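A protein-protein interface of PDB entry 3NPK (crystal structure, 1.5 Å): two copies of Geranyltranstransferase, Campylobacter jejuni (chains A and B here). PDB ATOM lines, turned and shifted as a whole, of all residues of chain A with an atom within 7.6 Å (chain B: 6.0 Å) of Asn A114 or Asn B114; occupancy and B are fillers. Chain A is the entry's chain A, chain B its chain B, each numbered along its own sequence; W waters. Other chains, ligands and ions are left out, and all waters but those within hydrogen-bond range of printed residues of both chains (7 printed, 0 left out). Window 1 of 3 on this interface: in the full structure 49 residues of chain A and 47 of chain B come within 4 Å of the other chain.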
ATOM      1  N   ALA A  68      -9.320   6.292   0.064  1.00  0.00           N
ATOM      2  CA  ALA A  68      -8.318   6.695   1.050  1.00  0.00           C
ATOM      3  C   ALA A  68      -8.430   5.859   2.334  1.00  0.00           C
ATOM      4  O   ALA A  68      -7.406   5.426   2.894  1.00  0.00           O
ATOM      5  CB  ALA A  68      -8.465   8.173   1.367  1.00  0.00           C
ATOM      6  N   PHE A  71      -7.045   2.469   1.659  1.00  0.00           N
ATOM      7  CA  PHE A  71      -5.578   2.522   1.564  1.00  0.00           C
ATOM      8  C   PHE A  71      -4.978   2.487   2.968  1.00  0.00           C
ATOM      9  O   PHE A  71      -4.004   1.769   3.210  1.00  0.00           O
ATOM     10  CB  PHE A  71      -5.087   3.784   0.839  1.00  0.00           C
ATOM     11  CG  PHE A  71      -5.201   3.737  -0.679  1.00  0.00           C
ATOM     12  CD1 PHE A  71      -5.809   2.683  -1.346  1.00  0.00           C
ATOM     13  CD2 PHE A  71      -4.708   4.787  -1.425  1.00  0.00           C
ATOM     14  CE1 PHE A  71      -5.902   2.678  -2.743  1.00  0.00           C
ATOM     15  CE2 PHE A  71      -4.797   4.804  -2.812  1.00  0.00           C
ATOM     16  CZ  PHE A  71      -5.398   3.743  -3.472  1.00  0.00           C
ATOM     17  N   ILE A  72      -5.524   3.288   3.881  1.00  0.00           N
ATOM     18  CA  ILE A  72      -5.032   3.292   5.255  1.00  0.00           C
ATOM     19  C   ILE A  72      -5.219   1.924   5.856  1.00  0.00           C
ATOM     20  O   ILE A  72      -4.312   1.386   6.483  1.00  0.00           O
ATOM     21  CB  ILE A  72      -5.806   4.305   6.131  1.00  0.00           C
ATOM     22  CG1 ILE A  72      -5.401   5.730   5.744  1.00  0.00           C
ATOM     23  CG2 ILE A  72      -5.615   4.006   7.654  1.00  0.00           C
ATOM     24  CD1 ILE A  72      -3.956   6.061   6.070  1.00  0.00           C
ATOM     25  N   HIS A  73      -6.408   1.366   5.696  1.00  0.00           N
ATOM     26  CA  HIS A  73      -6.683   0.078   6.308  1.00  0.00           C
ATOM     27  C   HIS A  73      -5.731  -0.998   5.769  1.00  0.00           C
ATOM     28  O   HIS A  73      -5.164  -1.790   6.534  1.00  0.00           O
ATOM     29  CB  HIS A  73      -8.149  -0.285   6.103  1.00  0.00           C
ATOM     30  CG  HIS A  73      -8.522  -1.586   6.721  1.00  0.00           C
ATOM     31  ND1 HIS A  73      -9.043  -2.638   6.003  1.00  0.00           N
ATOM     32  CD2 HIS A  73      -8.414  -2.014   7.999  1.00  0.00           C
ATOM     33  CE1 HIS A  73      -9.270  -3.653   6.820  1.00  0.00           C
ATOM     34  NE2 HIS A  73      -8.880  -3.304   8.034  1.00  0.00           N
ATOM     35  N   THR A  74      -5.564  -1.036   4.451  1.00  0.00           N
ATOM     36  CA  THR A  74      -4.667  -2.025   3.856  1.00  0.00           C
ATOM     37  C   THR A  74      -3.218  -1.835   4.305  1.00  0.00           C
ATOM     38  O   THR A  74      -2.530  -2.827   4.612  1.00  0.00           O
ATOM     39  CB  THR A  74      -4.796  -2.026   2.322  1.00  0.00           C
ATOM     40  OG1 THR A  74      -6.090  -2.520   1.972  1.00  0.00           O
ATOM     41  CG2 THR A  74      -3.734  -2.915   1.660  1.00  0.00           C
ATOM     42  N   TYR A  75      -2.742  -0.586   4.356  1.00  0.00           N
ATOM     43  CA  TYR A  75      -1.362  -0.367   4.827  1.00  0.00           C
ATOM     44  C   TYR A  75      -1.209  -0.937   6.244  1.00  0.00           C
ATOM     45  O   TYR A  75      -0.211  -1.596   6.567  1.00  0.00           O
ATOM     46  CB  TYR A  75      -0.923   1.113   4.731  1.00  0.00           C
ATOM     47  CG  TYR A  75      -0.608   1.785   6.065  1.00  0.00           C
ATOM     48  CD1 TYR A  75       0.537   1.454   6.789  1.00  0.00           C
ATOM     49  CD2 TYR A  75      -1.448   2.771   6.582  1.00  0.00           C
ATOM     50  CE1 TYR A  75       0.817   2.050   8.000  1.00  0.00           C
ATOM     51  CE2 TYR A  75      -1.162   3.391   7.791  1.00  0.00           C
ATOM     52  CZ  TYR A  75      -0.040   3.018   8.498  1.00  0.00           C
ATOM     53  OH  TYR A  75       0.261   3.597   9.711  1.00  0.00           O
ATOM     54  N   SER A  76      -2.225  -0.744   7.078  1.00  0.00           N
ATOM     55  CA  SER A  76      -2.116  -1.176   8.465  1.00  0.00           C
ATOM     56  C   SER A  76      -2.031  -2.691   8.554  1.00  0.00           C
ATOM     57  O   SER A  76      -1.305  -3.226   9.398  1.00  0.00           O
ATOM     58  CB  SER A  76      -3.277  -0.621   9.312  1.00  0.00           C
ATOM     59  OG  SER A  76      -4.483  -1.344   9.137  1.00  0.00           O
ATOM     60  N   HIS A  79       1.590  -3.773   7.504  1.00  0.00           N
ATOM     61  CA  HIS A  79       2.548  -3.594   8.601  1.00  0.00           C
ATOM     62  C   HIS A  79       2.281  -4.529   9.777  1.00  0.00           C
ATOM     63  O   HIS A  79       3.224  -5.097  10.340  1.00  0.00           O
ATOM     64  CB  HIS A  79       2.655  -2.133   9.042  1.00  0.00           C
ATOM     65  CG  HIS A  79       3.460  -1.290   8.101  1.00  0.00           C
ATOM     66  ND1 HIS A  79       3.855   0.000   8.401  1.00  0.00           N
ATOM     67  CD2 HIS A  79       3.987  -1.569   6.878  1.00  0.00           C
ATOM     68  CE1 HIS A  79       4.564   0.485   7.394  1.00  0.00           C
ATOM     69  NE2 HIS A  79       4.655  -0.446   6.457  1.00  0.00           N
ATOM     70  N   LEU A 108       7.820  -0.795   2.748  1.00  0.00           N
ATOM     71  CA  LEU A 108       7.681   0.358   1.844  1.00  0.00           C
ATOM     72  C   LEU A 108       6.318   0.454   1.151  1.00  0.00           C
ATOM     73  O   LEU A 108       5.830   1.561   0.918  1.00  0.00           O
ATOM     74  CB  LEU A 108       8.794   0.357   0.796  1.00  0.00           C
ATOM     75  CG  LEU A 108      10.209   0.522   1.368  1.00  0.00           C
ATOM     76  CD1 LEU A 108      11.255   0.420   0.240  1.00  0.00           C
ATOM     77  CD2 LEU A 108      10.324   1.846   2.153  1.00  0.00           C
ATOM     78  N   VAL A 109       5.716  -0.682   0.801  1.00  0.00           N
ATOM     79  CA  VAL A 109       4.367  -0.639   0.251  1.00  0.00           C
ATOM     80  C   VAL A 109       3.406  -0.055   1.297  1.00  0.00           C
ATOM     81  O   VAL A 109       2.574   0.793   0.970  1.00  0.00           O
ATOM     82  CB  VAL A 109       3.865  -2.021  -0.237  1.00  0.00           C
ATOM     83  CG1 VAL A 109       2.335  -1.993  -0.423  1.00  0.00           C
ATOM     84  CG2 VAL A 109       4.553  -2.430  -1.551  1.00  0.00           C
ATOM     85  N   GLY A 110       3.511  -0.497   2.550  1.00  0.00           N
ATOM     86  CA  GLY A 110       2.671   0.083   3.586  1.00  0.00           C
ATOM     87  C   GLY A 110       2.910   1.587   3.714  1.00  0.00           C
ATOM     88  O   GLY A 110       1.961   2.369   3.815  1.00  0.00           O
ATOM     89  N   ASP A 111       4.178   1.995   3.709  1.00  0.00           N
ATOM     90  CA  ASP A 111       4.524   3.420   3.805  1.00  0.00           C
ATOM     91  C   ASP A 111       3.883   4.182   2.646  1.00  0.00           C
ATOM     92  O   ASP A 111       3.289   5.255   2.843  1.00  0.00           O
ATOM     93  CB  ASP A 111       6.038   3.637   3.782  1.00  0.00           C
ATOM     94  CG  ASP A 111       6.719   3.173   5.064  1.00  0.00           C
ATOM     95  OD1 ASP A 111       6.023   2.879   6.054  1.00  0.00           O
ATOM     96  OD2 ASP A 111       7.954   3.092   5.078  1.00  0.00           O
ATOM     97  N   ALA A 112       4.012   3.631   1.437  1.00  0.00           N
ATOM     98  CA  ALA A 112       3.408   4.243   0.251  1.00  0.00           C
ATOM     99  C   ALA A 112       1.905   4.419   0.393  1.00  0.00           C
ATOM    100  O   ALA A 112       1.368   5.464   0.036  1.00  0.00           O
ATOM    101  CB  ALA A 112       3.743   3.436  -1.000  1.00  0.00           C
ATOM    102  N   LEU A 113       1.212   3.392   0.883  1.00  0.00           N
ATOM    103  CA  LEU A 113      -0.248   3.449   0.959  1.00  0.00           C
ATOM    104  C   LEU A 113      -0.716   4.446   2.028  1.00  0.00           C
ATOM    105  O   LEU A 113      -1.747   5.092   1.858  1.00  0.00           O
ATOM    106  CB  LEU A 113      -0.852   2.054   1.193  1.00  0.00           C
ATOM    107  CG  LEU A 113      -0.754   1.100  -0.011  1.00  0.00           C
ATOM    108  CD1 LEU A 113      -1.329  -0.284   0.360  1.00  0.00           C
ATOM    109  CD2 LEU A 113      -1.435   1.672  -1.267  1.00  0.00           C
ATOM    110  N   ASN A 114       0.021   4.536   3.135  1.00  0.00           N
ATOM    111  CA  ASN A 114      -0.264   5.513   4.187  1.00  0.00           C
ATOM    112  C   ASN A 114      -0.241   6.908   3.552  1.00  0.00           C
ATOM    113  O   ASN A 114      -1.217   7.659   3.612  1.00  0.00           O
ATOM    114  CB  ASN A 114       0.812   5.350   5.276  1.00  0.00           C
ATOM    115  CG  ASN A 114       0.575   6.200   6.522  1.00  0.00           C
ATOM    116  OD1 ASN A 114      -0.362   7.008   6.591  1.00  0.00           O
ATOM    117  ND2 ASN A 114       1.423   5.987   7.539  1.00  0.00           N
ATOM    118  N   THR A 115       0.866   7.248   2.901  1.00  0.00           N
ATOM    119  CA  THR A 115       0.984   8.576   2.278  1.00  0.00           C
ATOM    120  C   THR A 115      -0.012   8.757   1.137  1.00  0.00           C
ATOM    121  O   THR A 115      -0.593   9.839   0.968  1.00  0.00           O
ATOM    122  CB  THR A 115       2.416   8.794   1.778  1.00  0.00           C
ATOM    123  OG1 THR A 115       3.308   8.612   2.881  1.00  0.00           O
ATOM    124  CG2 THR A 115       2.611  10.195   1.203  1.00  0.00           C
ATOM    125  N   GLU A 116      -0.235   7.702   0.367  1.00  0.00           N
ATOM    126  CA  GLU A 116      -1.100   7.824  -0.809  1.00  0.00           C
ATOM    127  C   GLU A 116      -2.557   8.094  -0.426  1.00  0.00           C
ATOM    128  O   GLU A 116      -3.305   8.702  -1.200  1.00  0.00           O
ATOM    129  CB  GLU A 116      -1.007   6.575  -1.681  1.00  0.00           C
ATOM    130  CG  GLU A 116      -1.490   6.774  -3.110  1.00  0.00           C
ATOM    131  CD  GLU A 116      -0.550   7.600  -3.988  1.00  0.00           C
ATOM    132  OE1 GLU A 116       0.507   8.077  -3.517  1.00  0.00           O
ATOM    133  OE2 GLU A 116      -0.887   7.777  -5.178  1.00  0.00           O
ATOM    134  N   ALA A 117      -2.959   7.660   0.763  1.00  0.00           N
ATOM    135  CA  ALA A 117      -4.318   7.931   1.216  1.00  0.00           C
ATOM    136  C   ALA A 117      -4.544   9.444   1.214  1.00  0.00           C
ATOM    137  O   ALA A 117      -5.613   9.934   0.819  1.00  0.00           O
ATOM    138  CB  ALA A 117      -4.550   7.366   2.614  1.00  0.00           C
ATOM    139  N   PHE A 118      -3.527  10.178   1.656  1.00  0.00           N
ATOM    140  CA  PHE A 118      -3.635  11.629   1.699  1.00  0.00           C
ATOM    141  C   PHE A 118      -3.544  12.287   0.329  1.00  0.00           C
ATOM    142  O   PHE A 118      -4.207  13.301   0.087  1.00  0.00           O
ATOM    143  CB  PHE A 118      -2.676  12.204   2.737  1.00  0.00           C
ATOM    144  CG  PHE A 118      -2.996  11.709   4.097  1.00  0.00           C
ATOM    145  CD1 PHE A 118      -4.098  12.208   4.756  1.00  0.00           C
ATOM    146  CD2 PHE A 118      -2.310  10.632   4.660  1.00  0.00           C
ATOM    147  CE1 PHE A 118      -4.464  11.711   6.000  1.00  0.00           C
ATOM    148  CE2 PHE A 118      -2.681  10.119   5.890  1.00  0.00           C
ATOM    149  CZ  PHE A 118      -3.765  10.649   6.557  1.00  0.00           C
ATOM    150  N   LEU A 119      -2.735  11.724  -0.565  1.00  0.00           N
ATOM    151  CA  LEU A 119      -2.716  12.214  -1.941  1.00  0.00           C
ATOM    152  C   LEU A 119      -4.096  12.056  -2.583  1.00  0.00           C
ATOM    153  O   LEU A 119      -4.625  12.990  -3.183  1.00  0.00           O
ATOM    154  CB  LEU A 119      -1.652  11.493  -2.777  1.00  0.00           C
ATOM    155  CG  LEU A 119      -1.425  12.056  -4.184  1.00  0.00           C
ATOM    156  CD1 LEU A 119      -0.992  13.529  -4.127  1.00  0.00           C
ATOM    157  CD2 LEU A 119      -0.371  11.234  -4.902  1.00  0.00           C
ATOM    158  N   LEU A 138      -9.210  11.780   9.091  1.00  0.00           N
ATOM    159  CA  LEU A 138      -8.464  10.562   8.786  1.00  0.00           C
ATOM    160  C   LEU A 138      -7.125  10.518   9.511  1.00  0.00           C
ATOM    161  O   LEU A 138      -6.762   9.482  10.081  1.00  0.00           O
ATOM    162  CB  LEU A 138      -8.236  10.423   7.287  1.00  0.00           C
ATOM    163  CG  LEU A 138      -7.636   9.083   6.839  1.00  0.00           C
ATOM    164  CD1 LEU A 138      -8.546   7.915   7.220  1.00  0.00           C
ATOM    165  CD2 LEU A 138      -7.425   9.122   5.317  1.00  0.00           C
ATOM    166  N   ALA A 139      -6.371  11.617   9.487  1.00  0.00           N
ATOM    167  CA  ALA A 139      -5.032  11.593  10.093  1.00  0.00           C
ATOM    168  C   ALA A 139      -5.093  11.478  11.621  1.00  0.00           C
ATOM    169  O   ALA A 139      -4.218  10.875  12.240  1.00  0.00           O
ATOM    170  CB  ALA A 139      -4.215  12.821   9.683  1.00  0.00           C
ATOM    171  N   ALA A 142      -6.462   7.614  12.170  1.00  0.00           N
ATOM    172  CA  ALA A 142      -5.554   6.596  11.634  1.00  0.00           C
ATOM    173  C   ALA A 142      -4.146   6.698  12.190  1.00  0.00           C
ATOM    174  O   ALA A 142      -3.357   5.760  12.037  1.00  0.00           O
ATOM    175  CB  ALA A 142      -5.497   6.684  10.115  1.00  0.00           C
ATOM    176  N   GLY A 143      -3.826   7.827  12.815  1.00  0.00           N
ATOM    177  CA  GLY A 143      -2.469   8.078  13.256  1.00  0.00           C
ATOM    178  C   GLY A 143      -2.238   7.782  14.722  1.00  0.00           C
ATOM    179  O   GLY A 143      -2.900   6.900  15.303  1.00  0.00           O
ATOM    180  N   MET A 147      -5.449   4.633  15.512  1.00  0.00           N
ATOM    181  CA  MET A 147      -5.001   3.313  15.106  1.00  0.00           C
ATOM    182  C   MET A 147      -3.571   2.998  15.540  1.00  0.00           C
ATOM    183  O   MET A 147      -3.310   1.891  16.018  1.00  0.00           O
ATOM    184  CB  MET A 147      -5.134   3.198  13.593  1.00  0.00           C
ATOM    185  CG  MET A 147      -4.835   1.828  13.041  1.00  0.00           C
ATOM    186  SD  MET A 147      -5.017   1.897  11.089  1.00  0.00           S
ATOM    187  CE  MET A 147      -3.230   2.590  10.706  1.00  0.00           C
ATOM    188  N   VAL A 148      -2.643   3.938  15.362  1.00  0.00           N
ATOM    189  CA  VAL A 148      -1.249   3.598  15.636  1.00  0.00           C
ATOM    190  C   VAL A 148      -0.959   3.384  17.121  1.00  0.00           C
ATOM    191  O   VAL A 148      -0.255   2.437  17.480  1.00  0.00           O
ATOM    192  CB  VAL A 148      -0.259   4.599  15.023  1.00  0.00           C
ATOM    193  CG1 VAL A 148       1.196   4.185  15.386  1.00  0.00           C
ATOM    194  CG2 VAL A 148      -0.459   4.668  13.485  1.00  0.00           C
ATOM    195  N   PHE B  71       8.820  15.922   9.981  1.00  0.00           N
ATOM    196  CA  PHE B  71       8.171  14.667  10.384  1.00  0.00           C
ATOM    197  C   PHE B  71       8.349  13.598   9.293  1.00  0.00           C
ATOM    198  O   PHE B  71       8.672  12.440   9.599  1.00  0.00           O
ATOM    199  CB  PHE B  71       6.682  14.876  10.641  1.00  0.00           C
ATOM    200  CG  PHE B  71       6.358  15.498  11.982  1.00  0.00           C
ATOM    201  CD1 PHE B  71       7.349  16.015  12.800  1.00  0.00           C
ATOM    202  CD2 PHE B  71       5.036  15.618  12.384  1.00  0.00           C
ATOM    203  CE1 PHE B  71       7.022  16.615  14.029  1.00  0.00           C
ATOM    204  CE2 PHE B  71       4.704  16.203  13.610  1.00  0.00           C
ATOM    205  CZ  PHE B  71       5.703  16.713  14.427  1.00  0.00           C
ATOM    206  N   ILE B  72       8.096  13.967   8.028  1.00  0.00           N
ATOM    207  CA  ILE B  72       8.268  13.021   6.929  1.00  0.00           C
ATOM    208  C   ILE B  72       9.716  12.567   6.841  1.00  0.00           C
ATOM    209  O   ILE B  72      10.006  11.371   6.730  1.00  0.00           O
ATOM    210  CB  ILE B  72       7.873  13.644   5.565  1.00  0.00           C
ATOM    211  CG1 ILE B  72       6.360  13.797   5.479  1.00  0.00           C
ATOM    212  CG2 ILE B  72       8.420  12.798   4.380  1.00  0.00           C
ATOM    213  CD1 ILE B  72       5.610  12.456   5.486  1.00  0.00           C
ATOM    214  N   TYR B  75      10.575  10.201   9.743  1.00  0.00           N
ATOM    215  CA  TYR B  75       9.977   8.877   9.622  1.00  0.00           C
ATOM    216  C   TYR B  75      10.792   8.061   8.601  1.00  0.00           C
ATOM    217  O   TYR B  75      11.053   6.862   8.799  1.00  0.00           O
ATOM    218  CB  TYR B  75       8.469   8.949   9.251  1.00  0.00           C
ATOM    219  CG  TYR B  75       8.114   8.368   7.889  1.00  0.00           C
ATOM    220  CD1 TYR B  75       8.168   7.000   7.662  1.00  0.00           C
ATOM    221  CD2 TYR B  75       7.703   9.187   6.832  1.00  0.00           C
ATOM    222  CE1 TYR B  75       7.849   6.462   6.435  1.00  0.00           C
ATOM    223  CE2 TYR B  75       7.368   8.647   5.592  1.00  0.00           C
ATOM    224  CZ  TYR B  75       7.455   7.285   5.397  1.00  0.00           C
ATOM    225  OH  TYR B  75       7.166   6.733   4.172  1.00  0.00           O
ATOM    226  N   VAL B 109       6.506   4.098  15.150  1.00  0.00           N
ATOM    227  CA  VAL B 109       6.827   5.524  15.269  1.00  0.00           C
ATOM    228  C   VAL B 109       6.953   6.132  13.872  1.00  0.00           C
ATOM    229  O   VAL B 109       6.444   7.217  13.615  1.00  0.00           O
ATOM    230  CB  VAL B 109       8.126   5.771  16.082  1.00  0.00           C
ATOM    231  CG1 VAL B 109       8.665   7.190  15.848  1.00  0.00           C
ATOM    232  CG2 VAL B 109       7.875   5.497  17.561  1.00  0.00           C
ATOM    233  N   GLY B 110       7.613   5.438  12.953  1.00  0.00           N
ATOM    234  CA  GLY B 110       7.689   5.960  11.602  1.00  0.00           C
ATOM    235  C   GLY B 110       6.310   6.114  10.978  1.00  0.00           C
ATOM    236  O   GLY B 110       6.015   7.123  10.334  1.00  0.00           O
ATOM    237  N   ASP B 111       5.455   5.112  11.164  1.00  0.00           N
ATOM    238  CA  ASP B 111       4.098   5.168  10.633  1.00  0.00           C
ATOM    239  C   ASP B 111       3.350   6.373  11.196  1.00  0.00           C
ATOM    240  O   ASP B 111       2.646   7.096  10.459  1.00  0.00           O
ATOM    241  CB  ASP B 111       3.326   3.877  10.958  1.00  0.00           C
ATOM    242  CG  ASP B 111       3.812   2.682  10.163  1.00  0.00           C
ATOM    243  OD1 ASP B 111       4.580   2.875   9.191  1.00  0.00           O
ATOM    244  OD2 ASP B 111       3.392   1.553  10.503  1.00  0.00           O
ATOM    245  N   ALA B 112       3.480   6.563  12.503  1.00  0.00           N
ATOM    246  CA  ALA B 112       2.848   7.690  13.187  1.00  0.00           C
ATOM    247  C   ALA B 112       3.313   9.020  12.620  1.00  0.00           C
ATOM    248  O   ALA B 112       2.501   9.923  12.397  1.00  0.00           O
ATOM    249  CB  ALA B 112       3.136   7.633  14.676  1.00  0.00           C
ATOM    250  N   LEU B 113       4.611   9.152  12.363  1.00  0.00           N
ATOM    251  CA  LEU B 113       5.132  10.437  11.895  1.00  0.00           C
ATOM    252  C   LEU B 113       4.735  10.733  10.451  1.00  0.00           C
ATOM    253  O   LEU B 113       4.524  11.876  10.090  1.00  0.00           O
ATOM    254  CB  LEU B 113       6.644  10.539  12.052  1.00  0.00           C
ATOM    255  CG  LEU B 113       7.136  10.633  13.493  1.00  0.00           C
ATOM    256  CD1 LEU B 113       8.659  10.582  13.493  1.00  0.00           C
ATOM    257  CD2 LEU B 113       6.621  11.923  14.163  1.00  0.00           C
ATOM    258  N   ASN B 114       4.636   9.688   9.633  1.00  0.00           N
ATOM    259  CA  ASN B 114       4.162   9.817   8.263  1.00  0.00           C
ATOM    260  C   ASN B 114       2.745  10.420   8.293  1.00  0.00           C
ATOM    261  O   ASN B 114       2.479  11.470   7.702  1.00  0.00           O
ATOM    262  CB  ASN B 114       4.218   8.419   7.629  1.00  0.00           C
ATOM    263  CG  ASN B 114       3.854   8.396   6.136  1.00  0.00           C
ATOM    264  OD1 ASN B 114       3.511   9.415   5.527  1.00  0.00           O
ATOM    265  ND2 ASN B 114       3.943   7.201   5.542  1.00  0.00           N
ATOM    266  N   THR B 115       1.855   9.792   9.044  1.00  0.00           N
ATOM    267  CA  THR B 115       0.478  10.249   9.126  1.00  0.00           C
ATOM    268  C   THR B 115       0.400  11.614   9.810  1.00  0.00           C
ATOM    269  O   THR B 115      -0.368  12.490   9.390  1.00  0.00           O
ATOM    270  CB  THR B 115      -0.403   9.212   9.861  1.00  0.00           C
ATOM    271  OG1 THR B 115      -0.304   7.951   9.170  1.00  0.00           O
ATOM    272  CG2 THR B 115      -1.881   9.667   9.887  1.00  0.00           C
ATOM    273  N   GLU B 116       1.211  11.806  10.847  1.00  0.00           N
ATOM    274  CA  GLU B 116       1.134  13.048  11.623  1.00  0.00           C
ATOM    275  C   GLU B 116       1.548  14.267  10.798  1.00  0.00           C
ATOM    276  O   GLU B 116       1.076  15.371  11.041  1.00  0.00           O
ATOM    277  CB  GLU B 116       1.976  12.966  12.885  1.00  0.00           C
ATOM    278  CG  GLU B 116       1.606  14.032  13.913  1.00  0.00           C
ATOM    279  CD  GLU B 116       0.281  13.764  14.622  1.00  0.00           C
ATOM    280  OE1 GLU B 116      -0.422  12.765  14.312  1.00  0.00           O
ATOM    281  OE2 GLU B 116      -0.071  14.586  15.487  1.00  0.00           O
ATOM    282  N   ALA B 117       2.437  14.080   9.827  1.00  0.00           N
ATOM    283  CA  ALA B 117       2.796  15.185   8.943  1.00  0.00           C
ATOM    284  C   ALA B 117       1.537  15.775   8.304  1.00  0.00           C
ATOM    285  O   ALA B 117       1.411  16.999   8.159  1.00  0.00           O
ATOM    286  CB  ALA B 117       3.758  14.699   7.848  1.00  0.00           C
ATOM    287  N   PHE B 118       0.611  14.906   7.897  1.00  0.00           N
ATOM    288  CA  PHE B 118      -0.617  15.395   7.266  1.00  0.00           C
ATOM    289  C   PHE B 118      -1.613  15.994   8.251  1.00  0.00           C
ATOM    290  O   PHE B 118      -2.314  16.936   7.907  1.00  0.00           O
ATOM    291  CB  PHE B 118      -1.205  14.316   6.354  1.00  0.00           C
ATOM    292  CG  PHE B 118      -0.260  13.958   5.260  1.00  0.00           C
ATOM    293  CD1 PHE B 118      -0.098  14.814   4.177  1.00  0.00           C
ATOM    294  CD2 PHE B 118       0.565  12.847   5.358  1.00  0.00           C
ATOM    295  CE1 PHE B 118       0.831  14.545   3.183  1.00  0.00           C
ATOM    296  CE2 PHE B 118       1.505  12.569   4.364  1.00  0.00           C
ATOM    297  CZ  PHE B 118       1.639  13.415   3.270  1.00  0.00           C
HETATM  298  O   HOH W   1      -2.895  11.342  14.807  1.00  0.00           O
HETATM  299  O   HOH W   2       0.637   9.539   5.659  1.00  0.00           O
HETATM  300  O   HOH W   3      -1.280   5.710  10.270  1.00  0.00           O
HETATM  301  O   HOH W   4       9.350   5.019   3.481  1.00  0.00           O
HETATM  302  O   HOH W   5       5.995   8.345   2.439  1.00  0.00           O
HETATM  303  O   HOH W   6       0.701   1.386  11.525  1.00  0.00           O
HETATM  304  O   HOH W   7       4.060   4.604   7.123  1.00  0.00           O
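Tyr A75 touches Asp B111, and with the chains exchanged Asp A111 touches Tyr B75.
Asp A111 touches its own counterpart, Asp B111.
Asp A111 touches Asn B114, and with the chains exchanged Asn A114 touches Asp B111.
Thr A115 touches Phe B118, and with the chains exchanged Phe A118 touches Thr B115.
Of the 14 pairs that touch across the chains among the printed residues, 11 have their exchanged pair printed and touching as well.
OH of Tyr A75 lies within hydrogen-bond range of ND2 of Asn A114, at 3.4 Å.
The backbone carbonyl oxygen (O) of Gly A143 lies within hydrogen-bond range of the backbone NH (N) of Val A148 (3.0 Å).
The backbone carbonyl oxygen (O) of Asp A111 sits at hydrogen-bond distance from the side-chain hydroxyl (OG1) of Thr A115 (3.4 Å).
O of Asp B111 lies within hydrogen-bond range of OG1 of Thr B115, 3.3 Å away.
ND2 of Asn A114 lies within hydrogen-bond range of O of Asp B111 (3.4 Å).
A ring nitrogen (ND1) of His A79 is in hydrogen-bond range of the side-chain carboxylate of Asp B111.
OG1 of Thr A115 is in hydrogen-bond range of OD1 of Asn B114, 2.8 Å away.
The side-chain amide nitrogen (ND2) of Asn B114 is in hydrogen-bond range of the backbone carbonyl oxygen (O) of Asp A111, 3.4 Å away.
ND2 of Asn A114 lies close to ND2 of Asn B114, 3.4 Å away.
OD1 of Asp B111 lies close to OD1 of Asp A111 (3.5 Å).
OD1 of Asn A114 lies within hydrogen-bond range of OG1 of Thr B115, 2.7 Å away.
Printed residues of chain B that touch a printed residue of chain A: Tyr B75, Asp B111, Asn B114, Thr B115 and Phe B118.
Along chain B the printed residues that touch a printed residue of chain A span positions 75 to 118.
Along chain A the printed residues that touch a printed residue of chain B span positions 75 to 143.
Among the printed residues, 14 pairs touch across the chains.
Of chain B, only Asp B111 (3.4 Å), Asn B114 (3.4 Å) and Thr B115 (2.7 Å) come within 4 Å of Asn A114.
Asn B114 touches just these residues of chain A: Asp A111 (3.4 Å), Asn A114 (3.4 Å) and Thr A115 (2.8 Å).
Of the printed residues of chain B, Gly A143 touches Thr B115.
Printed residues of chain A within 4 Å of Thr B115: Asn A114 (2.7 Å), Phe A118 (3.95 Å), Ala A139 (3.5 Å) and Gly A143 (3.8 Å).
Printed residues of chain A within 4 Å of Phe B118: Thr A115 and Phe A118.
Printed residues of chain A within 4 Å of Tyr B75: Asp A111 (3.3 Å).
Printed residues of chain B within 4 Å of Asp A111: Tyr B75 (3.3 Å), Asp B111 (3.5 Å) and Asn B114 (3.4 Å).
The nearest residue of chain A that does not touch Asn B114 is Ala A112 (5.4 Å).
Water W3 lies within hydrogen-bond range of OH of Tyr A75 (2.7 Å), OG1 of Thr B115 (2.7 Å) and O of Ala A142 (2.7 Å).
Water W7 lies within hydrogen-bond range of OD1 of Asp B111, OD1 of Asp A111, ND2 of Asn A114 and ND2 of Asn B114.
Water W4 bridges the side-chain hydroxyl (OH) of Tyr B75 (2.9 Å) and the side-chain carboxylate (OD2) of Asp A111 (2.9 Å).
Water W2 bridges OD1 of Asn A114 (2.9 Å) and OD1 of Asn B114 (2.9 Å).
Water W6 bridges the side-chain carboxylate (OD2) of Asp B111 and the side-chain hydroxyl (OH) of Tyr A75.
Water W1 lies within hydrogen-bond range of OE1 of Glu B116 and O of Ala A139.
Among the printed residues, merely in contact across the chains: Tyr A75 with Asp B111, Asp A111 with Tyr B75, Thr A115 with Phe B118, Phe A118 with Thr B115, Phe A118 with Phe B118, Ala A139 with Thr B115 and Gly A143 with Thr B115.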
